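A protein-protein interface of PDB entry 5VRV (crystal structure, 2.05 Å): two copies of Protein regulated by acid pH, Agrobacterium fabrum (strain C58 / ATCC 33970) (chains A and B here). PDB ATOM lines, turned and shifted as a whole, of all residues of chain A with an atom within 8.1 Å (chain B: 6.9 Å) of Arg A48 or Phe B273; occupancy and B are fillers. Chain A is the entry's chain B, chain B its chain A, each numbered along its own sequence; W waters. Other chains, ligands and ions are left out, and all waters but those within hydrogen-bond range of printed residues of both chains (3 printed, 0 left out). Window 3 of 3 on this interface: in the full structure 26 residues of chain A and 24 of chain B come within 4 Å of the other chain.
The side-chain carboxylate of Glu B277 is in salt-bridge range of the guanidinium group of Arg A48, 2.8 Å away. The side-chain carboxylate (OE1) of Glu B274 lies within salt-bridge range of the guanidinium group (NH2) of Arg A80. The guanidinium group of Arg B278 lies within salt-bridge range of the side-chain carboxylate of Asp A315 (2.8 Å).
O of Arg A80 is in hydrogen-bond range of N of Trp A50. The guanidinium group (NH1) of Arg A80 lies within salt-bridge range of the side-chain carboxylate (OD2) of Asp A315, at 3.5 Å. The guanidinium group (NE) of Arg A80 lies within salt-bridge range of the side-chain carboxylate (OD1) of Asp A308, 3.7 Å away. The side-chain hydroxyl (OG) of Ser A49 lies within hydrogen-bond range of the guanidinium group (NH1) of Arg A80, at 2.9 Å. O of Arg A48 lies within hydrogen-bond range of N of Arg A80, at 2.9 Å. The side-chain hydroxyl (OG) of Ser A49 lies within hydrogen-bond range of the side-chain carboxylate (OD2) of Asp A315, at 2.4 Å.
Among the printed residues, pairs that only touch across the chains: Arg A48 with Phe B273 (3.5 Å), Leu A311 with Glu B274 (3.6 Å) and Asp A315 with Glu B274 (3.8 Å).
Arg A48 touches two residues of chain B. Printed residues of chain B within 4 Å of Arg A80: Glu B274. Ser B254 touches none of the printed residues of chain A. Of chain A, only Arg A48 (3.5 Å) comes within 4 Å of Phe B273. Of the printed residues of chain A, Glu B274 touches Arg A80, Leu A311 and Asp A315. Of the printed residues of chain A, Glu B277 touches Arg A48. The nearest printed residue of chain A that does not touch Arg B278 is Gln A46 (4.4 Å).
Of the 18 printed residues of chain A, 4 touch a printed residue of chain B. Hydrophobic or aromatic side chains of chain A within 4 Å of the printed part of chain B: Leu A311. Of the 16 printed residues of chain B, 4 touch a printed residue of chain A. Hydrophobic or aromatic side chains of chain B within 4 Å of the printed part of chain A: Phe B273.
No position is printed for both chains.
Water W2 lies within hydrogen-bond range of OE2 of Glu B274 (2.6 Å), OD2 of Asp A315 (2.8 Å) and N of Arg A48 (3.0 Å). Water W3 lies within hydrogen-bond range of NE of Arg B278, NE2 of Gln A46 and OD1 of Asp A315. Water W1 lies within hydrogen-bond range of OE2 of Glu B274 (2.8 Å), NH1 of Arg B278 (2.9 Å) and O of Leu A311 (3.0 Å).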
ATOM      1  N   ILE A  45      17.078 -33.060  22.419  1.00  0.00           N
ATOM      2  CA  ILE A  45      15.962 -32.738  23.305  1.00  0.00           C
ATOM      3  C   ILE A  45      16.174 -31.336  23.823  1.00  0.00           C
ATOM      4  O   ILE A  45      17.151 -31.080  24.524  1.00  0.00           O
ATOM      5  CB  ILE A  45      15.882 -33.692  24.520  1.00  0.00           C
ATOM      6  CG1 ILE A  45      15.509 -35.106  24.047  1.00  0.00           C
ATOM      7  CG2 ILE A  45      14.849 -33.188  25.550  1.00  0.00           C
ATOM      8  CD1 ILE A  45      15.482 -36.158  25.137  1.00  0.00           C
ATOM      9  N   GLN A  46      15.246 -30.439  23.512  1.00  0.00           N
ATOM     10  CA  GLN A  46      15.358 -29.054  23.938  1.00  0.00           C
ATOM     11  C   GLN A  46      13.977 -28.516  24.209  1.00  0.00           C
ATOM     12  O   GLN A  46      13.110 -28.550  23.339  1.00  0.00           O
ATOM     13  CB  GLN A  46      16.062 -28.215  22.859  1.00  0.00           C
ATOM     14  CG  GLN A  46      16.235 -26.730  23.196  1.00  0.00           C
ATOM     15  CD  GLN A  46      17.104 -26.478  24.416  1.00  0.00           C
ATOM     16  OE1 GLN A  46      18.100 -27.162  24.630  1.00  0.00           O
ATOM     17  NE2 GLN A  46      16.751 -25.468  25.202  1.00  0.00           N
ATOM     18  N   GLY A  47      13.787 -28.018  25.425  1.00  0.00           N
ATOM     19  CA  GLY A  47      12.514 -27.481  25.834  1.00  0.00           C
ATOM     20  C   GLY A  47      11.434 -28.530  25.694  1.00  0.00           C
ATOM     21  O   GLY A  47      11.612 -29.672  26.119  1.00  0.00           O
ATOM     22  N   ARG A  48      10.328 -28.140  25.074  1.00  0.00           N
ATOM     23  CA  ARG A  48       9.197 -29.033  24.863  1.00  0.00           C
ATOM     24  C   ARG A  48       9.270 -29.673  23.479  1.00  0.00           C
ATOM     25  O   ARG A  48       8.245 -30.010  22.922  1.00  0.00           O
ATOM     26  CB  ARG A  48       7.872 -28.271  25.046  1.00  0.00           C
ATOM     27  CG  ARG A  48       7.635 -27.765  26.464  1.00  0.00           C
ATOM     28  CD  ARG A  48       6.308 -27.038  26.578  1.00  0.00           C
ATOM     29  NE  ARG A  48       6.052 -26.540  27.938  1.00  0.00           N
ATOM     30  CZ  ARG A  48       5.259 -27.101  28.854  1.00  0.00           C
ATOM     31  NH1 ARG A  48       4.558 -28.203  28.597  1.00  0.00           N
ATOM     32  NH2 ARG A  48       5.136 -26.526  30.053  1.00  0.00           N
ATOM     33  N   SER A  49      10.481 -29.856  22.943  1.00  0.00           N
ATOM     34  CA  SER A  49      10.657 -30.478  21.627  1.00  0.00           C
ATOM     35  C   SER A  49      11.768 -31.529  21.592  1.00  0.00           C
ATOM     36  O   SER A  49      12.833 -31.356  22.224  1.00  0.00           O
ATOM     37  CB  SER A  49      11.037 -29.433  20.560  1.00  0.00           C
ATOM     38  OG  SER A  49      10.203 -28.292  20.592  1.00  0.00           O
ATOM     39  N   TRP A  50      11.492 -32.599  20.840  1.00  0.00           N
ATOM     40  CA  TRP A  50      12.432 -33.678  20.501  1.00  0.00           C
ATOM     41  C   TRP A  50      12.617 -33.424  19.011  1.00  0.00           C
ATOM     42  O   TRP A  50      11.646 -33.465  18.252  1.00  0.00           O
ATOM     43  CB  TRP A  50      11.834 -35.075  20.720  1.00  0.00           C
ATOM     44  CG  TRP A  50      11.886 -35.552  22.105  1.00  0.00           C
ATOM     45  CD1 TRP A  50      11.667 -34.815  23.235  1.00  0.00           C
ATOM     46  CD2 TRP A  50      12.066 -36.905  22.535  1.00  0.00           C
ATOM     47  NE1 TRP A  50      11.769 -35.614  24.347  1.00  0.00           N
ATOM     48  CE2 TRP A  50      12.008 -36.905  23.946  1.00  0.00           C
ATOM     49  CE3 TRP A  50      12.302 -38.114  21.868  1.00  0.00           C
ATOM     50  CZ2 TRP A  50      12.166 -38.081  24.709  1.00  0.00           C
ATOM     51  CZ3 TRP A  50      12.472 -39.284  22.627  1.00  0.00           C
ATOM     52  CH2 TRP A  50      12.402 -39.253  24.033  1.00  0.00           C
ATOM     53  N   ILE A  51      13.845 -33.146  18.599  1.00  0.00           N
ATOM     54  CA  ILE A  51      14.140 -32.819  17.207  1.00  0.00           C
ATOM     55  C   ILE A  51      15.098 -33.830  16.621  1.00  0.00           C
ATOM     56  O   ILE A  51      16.240 -33.931  17.057  1.00  0.00           O
ATOM     57  CB  ILE A  51      14.724 -31.395  17.111  1.00  0.00           C
ATOM     58  CG1 ILE A  51      13.739 -30.407  17.755  1.00  0.00           C
ATOM     59  CG2 ILE A  51      15.010 -30.998  15.664  1.00  0.00           C
ATOM     60  CD1 ILE A  51      14.199 -28.978  17.735  1.00  0.00           C
ATOM     61  N   ALA A  74       8.460 -39.272  22.010  1.00  0.00           N
ATOM     62  CA  ALA A  74       8.299 -37.837  22.291  1.00  0.00           C
ATOM     63  C   ALA A  74       6.906 -37.552  22.893  1.00  0.00           C
ATOM     64  O   ALA A  74       6.779 -36.710  23.785  1.00  0.00           O
ATOM     65  CB  ALA A  74       8.521 -37.014  21.041  1.00  0.00           C
ATOM     66  N   ALA A  77       6.909 -38.431  26.524  1.00  0.00           N
ATOM     67  CA  ALA A  77       7.680 -37.502  27.359  1.00  0.00           C
ATOM     68  C   ALA A  77       6.984 -36.137  27.501  1.00  0.00           C
ATOM     69  O   ALA A  77       7.463 -35.270  28.232  1.00  0.00           O
ATOM     70  CB  ALA A  77       9.075 -37.318  26.775  1.00  0.00           C
ATOM     71  N   GLY A  78       5.863 -35.954  26.804  1.00  0.00           N
ATOM     72  CA  GLY A  78       5.105 -34.706  26.835  1.00  0.00           C
ATOM     73  C   GLY A  78       5.706 -33.670  25.898  1.00  0.00           C
ATOM     74  O   GLY A  78       5.516 -32.471  26.101  1.00  0.00           O
ATOM     75  N   ALA A  79       6.394 -34.131  24.853  1.00  0.00           N
ATOM     76  CA  ALA A  79       7.061 -33.228  23.919  1.00  0.00           C
ATOM     77  C   ALA A  79       6.560 -33.327  22.495  1.00  0.00           C
ATOM     78  O   ALA A  79       6.058 -34.369  22.074  1.00  0.00           O
ATOM     79  CB  ALA A  79       8.559 -33.523  23.925  1.00  0.00           C
ATOM     80  N   ARG A  80       6.725 -32.235  21.745  1.00  0.00           N
ATOM     81  CA  ARG A  80       6.379 -32.243  20.342  1.00  0.00           C
ATOM     82  C   ARG A  80       7.545 -32.957  19.641  1.00  0.00           C
ATOM     83  O   ARG A  80       8.711 -32.828  20.050  1.00  0.00           O
ATOM     84  CB  ARG A  80       6.169 -30.824  19.775  1.00  0.00           C
ATOM     85  CG  ARG A  80       7.413 -29.959  19.658  1.00  0.00           C
ATOM     86  CD  ARG A  80       7.112 -28.601  19.015  1.00  0.00           C
ATOM     87  NE  ARG A  80       6.185 -27.815  19.812  1.00  0.00           N
ATOM     88  CZ  ARG A  80       6.525 -26.979  20.795  1.00  0.00           C
ATOM     89  NH1 ARG A  80       7.804 -26.770  21.135  1.00  0.00           N
ATOM     90  NH2 ARG A  80       5.571 -26.343  21.433  1.00  0.00           N
ATOM     91  N   ALA A  81       7.225 -33.727  18.610  1.00  0.00           N
ATOM     92  CA  ALA A  81       8.224 -34.433  17.832  1.00  0.00           C
ATOM     93  C   ALA A  81       8.404 -33.635  16.558  1.00  0.00           C
ATOM     94  O   ALA A  81       7.426 -33.172  15.978  1.00  0.00           O
ATOM     95  CB  ALA A  81       7.747 -35.833  17.505  1.00  0.00           C
ATOM     96  N   ALA A  82       9.650 -33.458  16.133  1.00  0.00           N
ATOM     97  CA  ALA A  82       9.947 -32.713  14.916  1.00  0.00           C
ATOM     98  C   ALA A  82      11.131 -33.340  14.221  1.00  0.00           C
ATOM     99  O   ALA A  82      12.029 -33.867  14.877  1.00  0.00           O
ATOM    100  CB  ALA A  82      10.266 -31.265  15.254  1.00  0.00           C
ATOM    101  N   ASP A 308       3.302 -25.199  15.610  1.00  0.00           N
ATOM    102  CA  ASP A 308       4.460 -25.912  16.134  1.00  0.00           C
ATOM    103  C   ASP A 308       5.725 -25.661  15.339  1.00  0.00           C
ATOM    104  O   ASP A 308       6.818 -25.832  15.890  1.00  0.00           O
ATOM    105  CB  ASP A 308       4.241 -27.431  16.135  1.00  0.00           C
ATOM    106  CG  ASP A 308       3.255 -27.894  17.175  1.00  0.00           C
ATOM    107  OD1 ASP A 308       2.931 -27.123  18.109  1.00  0.00           O
ATOM    108  OD2 ASP A 308       2.819 -29.065  17.063  1.00  0.00           O
ATOM    109  N   LEU A 311       7.776 -22.860  16.802  1.00  0.00           N
ATOM    110  CA  LEU A 311       8.199 -23.296  18.136  1.00  0.00           C
ATOM    111  C   LEU A 311       9.318 -24.340  18.061  1.00  0.00           C
ATOM    112  O   LEU A 311      10.340 -24.218  18.752  1.00  0.00           O
ATOM    113  CB  LEU A 311       7.023 -23.817  18.965  1.00  0.00           C
ATOM    114  CG  LEU A 311       5.926 -22.787  19.250  1.00  0.00           C
ATOM    115  CD1 LEU A 311       4.723 -23.420  19.945  1.00  0.00           C
ATOM    116  CD2 LEU A 311       6.484 -21.625  20.063  1.00  0.00           C
ATOM    117  N   ALA A 312       9.131 -25.341  17.213  1.00  0.00           N
ATOM    118  CA  ALA A 312      10.113 -26.400  17.052  1.00  0.00           C
ATOM    119  C   ALA A 312      11.417 -25.849  16.501  1.00  0.00           C
ATOM    120  O   ALA A 312      12.495 -26.220  16.971  1.00  0.00           O
ATOM    121  CB  ALA A 312       9.590 -27.491  16.142  1.00  0.00           C
ATOM    122  N   ASP A 315      13.457 -24.253  19.121  1.00  0.00           N
ATOM    123  CA  ASP A 315      14.192 -25.258  19.926  1.00  0.00           C
ATOM    124  C   ASP A 315      15.414 -25.796  19.151  1.00  0.00           C
ATOM    125  O   ASP A 315      16.483 -25.979  19.731  1.00  0.00           O
ATOM    126  CB  ASP A 315      13.269 -26.384  20.419  1.00  0.00           C
ATOM    127  CG  ASP A 315      12.357 -25.931  21.569  1.00  0.00           C
ATOM    128  OD1 ASP A 315      12.832 -25.188  22.448  1.00  0.00           O
ATOM    129  OD2 ASP A 315      11.197 -26.358  21.626  1.00  0.00           O
ATOM    130  N   LEU B 104       7.402 -10.151  29.276  1.00  0.00           N
ATOM    131  CA  LEU B 104       8.217 -11.368  29.180  1.00  0.00           C
ATOM    132  C   LEU B 104       8.150 -12.246  30.407  1.00  0.00           C
ATOM    133  O   LEU B 104       8.350 -13.434  30.309  1.00  0.00           O
ATOM    134  CB  LEU B 104       9.689 -11.016  29.020  1.00  0.00           C
ATOM    135  CG  LEU B 104      10.182 -10.465  27.704  1.00  0.00           C
ATOM    136  CD1 LEU B 104      11.542  -9.840  27.908  1.00  0.00           C
ATOM    137  CD2 LEU B 104      10.229 -11.575  26.678  1.00  0.00           C
ATOM    138  N   PRO B 252       9.232 -17.085  34.907  1.00  0.00           N
ATOM    139  CA  PRO B 252       8.145 -17.069  33.942  1.00  0.00           C
ATOM    140  C   PRO B 252       6.864 -16.660  34.644  1.00  0.00           C
ATOM    141  O   PRO B 252       6.805 -16.657  35.880  1.00  0.00           O
ATOM    142  CB  PRO B 252       8.065 -18.525  33.456  1.00  0.00           C
ATOM    143  CG  PRO B 252       9.330 -19.168  33.898  1.00  0.00           C
ATOM    144  CD  PRO B 252       9.714 -18.454  35.149  1.00  0.00           C
ATOM    145  N   MET B 253       5.853 -16.293  33.879  1.00  0.00           N
ATOM    146  CA  MET B 253       4.573 -15.865  34.460  1.00  0.00           C
ATOM    147  C   MET B 253       3.836 -17.044  35.050  1.00  0.00           C
ATOM    148  O   MET B 253       4.079 -18.194  34.663  1.00  0.00           O
ATOM    149  CB  MET B 253       3.727 -15.201  33.372  1.00  0.00           C
ATOM    150  CG  MET B 253       4.430 -13.949  32.844  1.00  0.00           C
ATOM    151  SD  MET B 253       3.455 -13.195  31.307  1.00  0.00           S
ATOM    152  CE  MET B 253       4.606 -13.846  29.850  1.00  0.00           C
ATOM    153  N   SER B 254       2.947 -16.776  36.006  1.00  0.00           N
ATOM    154  CA  SER B 254       2.144 -17.836  36.628  1.00  0.00           C
ATOM    155  C   SER B 254       0.789 -17.922  35.942  1.00  0.00           C
ATOM    156  O   SER B 254       0.701 -18.292  34.772  1.00  0.00           O
ATOM    157  CB  SER B 254       1.965 -17.584  38.118  1.00  0.00           C
ATOM    158  OG  SER B 254       1.369 -16.326  38.348  1.00  0.00           O
ATOM    159  N   ILE B 268       2.172 -15.388  19.696  1.00  0.00           N
ATOM    160  CA  ILE B 268       3.276 -14.747  20.415  1.00  0.00           C
ATOM    161  C   ILE B 268       3.218 -15.161  21.901  1.00  0.00           C
ATOM    162  O   ILE B 268       4.239 -15.175  22.577  1.00  0.00           O
ATOM    163  CB  ILE B 268       3.305 -13.209  20.198  1.00  0.00           C
ATOM    164  CG1 ILE B 268       4.515 -12.559  20.889  1.00  0.00           C
ATOM    165  CG2 ILE B 268       2.026 -12.555  20.688  1.00  0.00           C
ATOM    166  CD1 ILE B 268       5.855 -13.083  20.427  1.00  0.00           C
ATOM    167  N   GLY B 269       2.026 -15.535  22.379  1.00  0.00           N
ATOM    168  CA  GLY B 269       1.847 -16.012  23.758  1.00  0.00           C
ATOM    169  C   GLY B 269       2.554 -17.352  24.006  1.00  0.00           C
ATOM    170  O   GLY B 269       3.160 -17.556  25.063  1.00  0.00           O
ATOM    171  N   SER B 270       2.470 -18.262  23.030  1.00  0.00           N
ATOM    172  CA  SER B 270       3.136 -19.570  23.119  1.00  0.00           C
ATOM    173  C   SER B 270       4.647 -19.395  23.108  1.00  0.00           C
ATOM    174  O   SER B 270       5.385 -20.080  23.833  1.00  0.00           O
ATOM    175  CB  SER B 270       2.769 -20.429  21.916  1.00  0.00           C
ATOM    176  OG  SER B 270       1.378 -20.591  21.831  1.00  0.00           O
ATOM    177  N   THR B 271       5.079 -18.471  22.254  1.00  0.00           N
ATOM    178  CA  THR B 271       6.481 -18.152  22.068  1.00  0.00           C
ATOM    179  C   THR B 271       7.093 -17.603  23.360  1.00  0.00           C
ATOM    180  O   THR B 271       8.173 -18.041  23.763  1.00  0.00           O
ATOM    181  CB  THR B 271       6.643 -17.144  20.922  1.00  0.00           C
ATOM    182  OG1 THR B 271       5.935 -17.622  19.786  1.00  0.00           O
ATOM    183  CG2 THR B 271       8.065 -16.984  20.545  1.00  0.00           C
ATOM    184  N   LEU B 272       6.401 -16.648  23.989  1.00  0.00           N
ATOM    185  CA  LEU B 272       6.848 -16.035  25.255  1.00  0.00           C
ATOM    186  C   LEU B 272       6.892 -17.051  26.378  1.00  0.00           C
ATOM    187  O   LEU B 272       7.804 -17.038  27.191  1.00  0.00           O
ATOM    188  CB  LEU B 272       5.934 -14.871  25.662  1.00  0.00           C
ATOM    189  CG  LEU B 272       5.984 -13.617  24.781  1.00  0.00           C
ATOM    190  CD1 LEU B 272       4.877 -12.640  25.168  1.00  0.00           C
ATOM    191  CD2 LEU B 272       7.339 -12.949  24.871  1.00  0.00           C
ATOM    192  N   PHE B 273       5.893 -17.918  26.413  1.00  0.00           N
ATOM    193  CA  PHE B 273       5.817 -18.971  27.412  1.00  0.00           C
ATOM    194  C   PHE B 273       7.024 -19.916  27.322  1.00  0.00           C
ATOM    195  O   PHE B 273       7.633 -20.229  28.335  1.00  0.00           O
ATOM    196  CB  PHE B 273       4.503 -19.752  27.241  1.00  0.00           C
ATOM    197  CG  PHE B 273       4.364 -20.946  28.162  1.00  0.00           C
ATOM    198  CD1 PHE B 273       4.063 -20.772  29.521  1.00  0.00           C
ATOM    199  CD2 PHE B 273       4.494 -22.248  27.667  1.00  0.00           C
ATOM    200  CE1 PHE B 273       3.932 -21.869  30.366  1.00  0.00           C
ATOM    201  CE2 PHE B 273       4.361 -23.348  28.511  1.00  0.00           C
ATOM    202  CZ  PHE B 273       4.076 -23.158  29.860  1.00  0.00           C
ATOM    203  N   GLU B 274       7.374 -20.358  26.111  1.00  0.00           N
ATOM    204  CA  GLU B 274       8.515 -21.276  25.951  1.00  0.00           C
ATOM    205  C   GLU B 274       9.843 -20.565  26.135  1.00  0.00           C
ATOM    206  O   GLU B 274      10.822 -21.184  26.520  1.00  0.00           O
ATOM    207  CB  GLU B 274       8.437 -22.070  24.638  1.00  0.00           C
ATOM    208  CG  GLU B 274       7.276 -23.052  24.660  1.00  0.00           C
ATOM    209  CD  GLU B 274       7.199 -23.978  23.466  1.00  0.00           C
ATOM    210  OE1 GLU B 274       6.074 -24.438  23.169  1.00  0.00           O
ATOM    211  OE2 GLU B 274       8.225 -24.252  22.817  1.00  0.00           O
ATOM    212  N   HIS B 275       9.872 -19.263  25.860  1.00  0.00           N
ATOM    213  CA  HIS B 275      11.089 -18.470  26.089  1.00  0.00           C
ATOM    214  C   HIS B 275      11.361 -18.417  27.585  1.00  0.00           C
ATOM    215  O   HIS B 275      12.501 -18.545  28.030  1.00  0.00           O
ATOM    216  CB  HIS B 275      10.917 -17.050  25.563  1.00  0.00           C
ATOM    217  CG  HIS B 275      12.060 -16.152  25.889  1.00  0.00           C
ATOM    218  ND1 HIS B 275      13.187 -16.075  25.108  1.00  0.00           N
ATOM    219  CD2 HIS B 275      12.254 -15.299  26.918  1.00  0.00           C
ATOM    220  CE1 HIS B 275      14.028 -15.204  25.640  1.00  0.00           C
ATOM    221  NE2 HIS B 275      13.495 -14.739  26.751  1.00  0.00           N
ATOM    222  N   GLY B 276      10.295 -18.217  28.355  1.00  0.00           N
ATOM    223  CA  GLY B 276      10.402 -18.173  29.825  1.00  0.00           C
ATOM    224  C   GLY B 276      11.008 -19.437  30.410  1.00  0.00           C
ATOM    225  O   GLY B 276      11.977 -19.376  31.176  1.00  0.00           O
ATOM    226  N   GLU B 277      10.472 -20.589  30.024  1.00  0.00           N
ATOM    227  CA  GLU B 277      10.988 -21.872  30.506  1.00  0.00           C
ATOM    228  C   GLU B 277      12.421 -22.127  30.050  1.00  0.00           C
ATOM    229  O   GLU B 277      13.209 -22.734  30.763  1.00  0.00           O
ATOM    230  CB  GLU B 277      10.104 -23.023  30.038  1.00  0.00           C
ATOM    231  CG  GLU B 277       8.692 -22.999  30.606  1.00  0.00           C
ATOM    232  CD  GLU B 277       7.882 -24.231  30.217  1.00  0.00           C
ATOM    233  OE1 GLU B 277       8.359 -25.053  29.389  1.00  0.00           O
ATOM    234  OE2 GLU B 277       6.750 -24.379  30.732  1.00  0.00           O
ATOM    235  N   ARG B 278      12.741 -21.647  28.855  1.00  0.00           N
ATOM    236  CA  ARG B 278      14.068 -21.816  28.262  1.00  0.00           C
ATOM    237  C   ARG B 278      15.205 -21.065  28.991  1.00  0.00           C
ATOM    238  O   ARG B 278      16.323 -21.592  29.102  1.00  0.00           O
ATOM    239  CB  ARG B 278      13.990 -21.387  26.785  1.00  0.00           C
ATOM    240  CG  ARG B 278      15.272 -21.428  25.973  1.00  0.00           C
ATOM    241  CD  ARG B 278      15.034 -21.019  24.517  1.00  0.00           C
ATOM    242  NE  ARG B 278      14.066 -21.907  23.862  1.00  0.00           N
ATOM    243  CZ  ARG B 278      12.860 -21.568  23.391  1.00  0.00           C
ATOM    244  NH1 ARG B 278      12.103 -22.503  22.857  1.00  0.00           N
ATOM    245  NH2 ARG B 278      12.405 -20.311  23.409  1.00  0.00           N
ATOM    246  N   LEU B 313      12.713 -12.145  19.135  1.00  0.00           N
ATOM    247  CA  LEU B 313      12.962 -13.050  20.246  1.00  0.00           C
ATOM    248  C   LEU B 313      13.839 -14.225  19.777  1.00  0.00           C
ATOM    249  O   LEU B 313      14.681 -14.717  20.532  1.00  0.00           O
ATOM    250  CB  LEU B 313      11.635 -13.511  20.848  1.00  0.00           C
ATOM    251  CG  LEU B 313      11.649 -14.015  22.284  1.00  0.00           C
ATOM    252  CD1 LEU B 313      12.321 -13.014  23.213  1.00  0.00           C
ATOM    253  CD2 LEU B 313      10.215 -14.259  22.715  1.00  0.00           C
HETATM  254  O   HOH W   1       9.765 -22.612  21.195  1.00  0.00           O
HETATM  255  O   HOH W   2      10.272 -25.277  24.059  1.00  0.00           O
HETATM  256  O   HOH W   3      14.218 -24.449  24.836  1.00  0.00           O
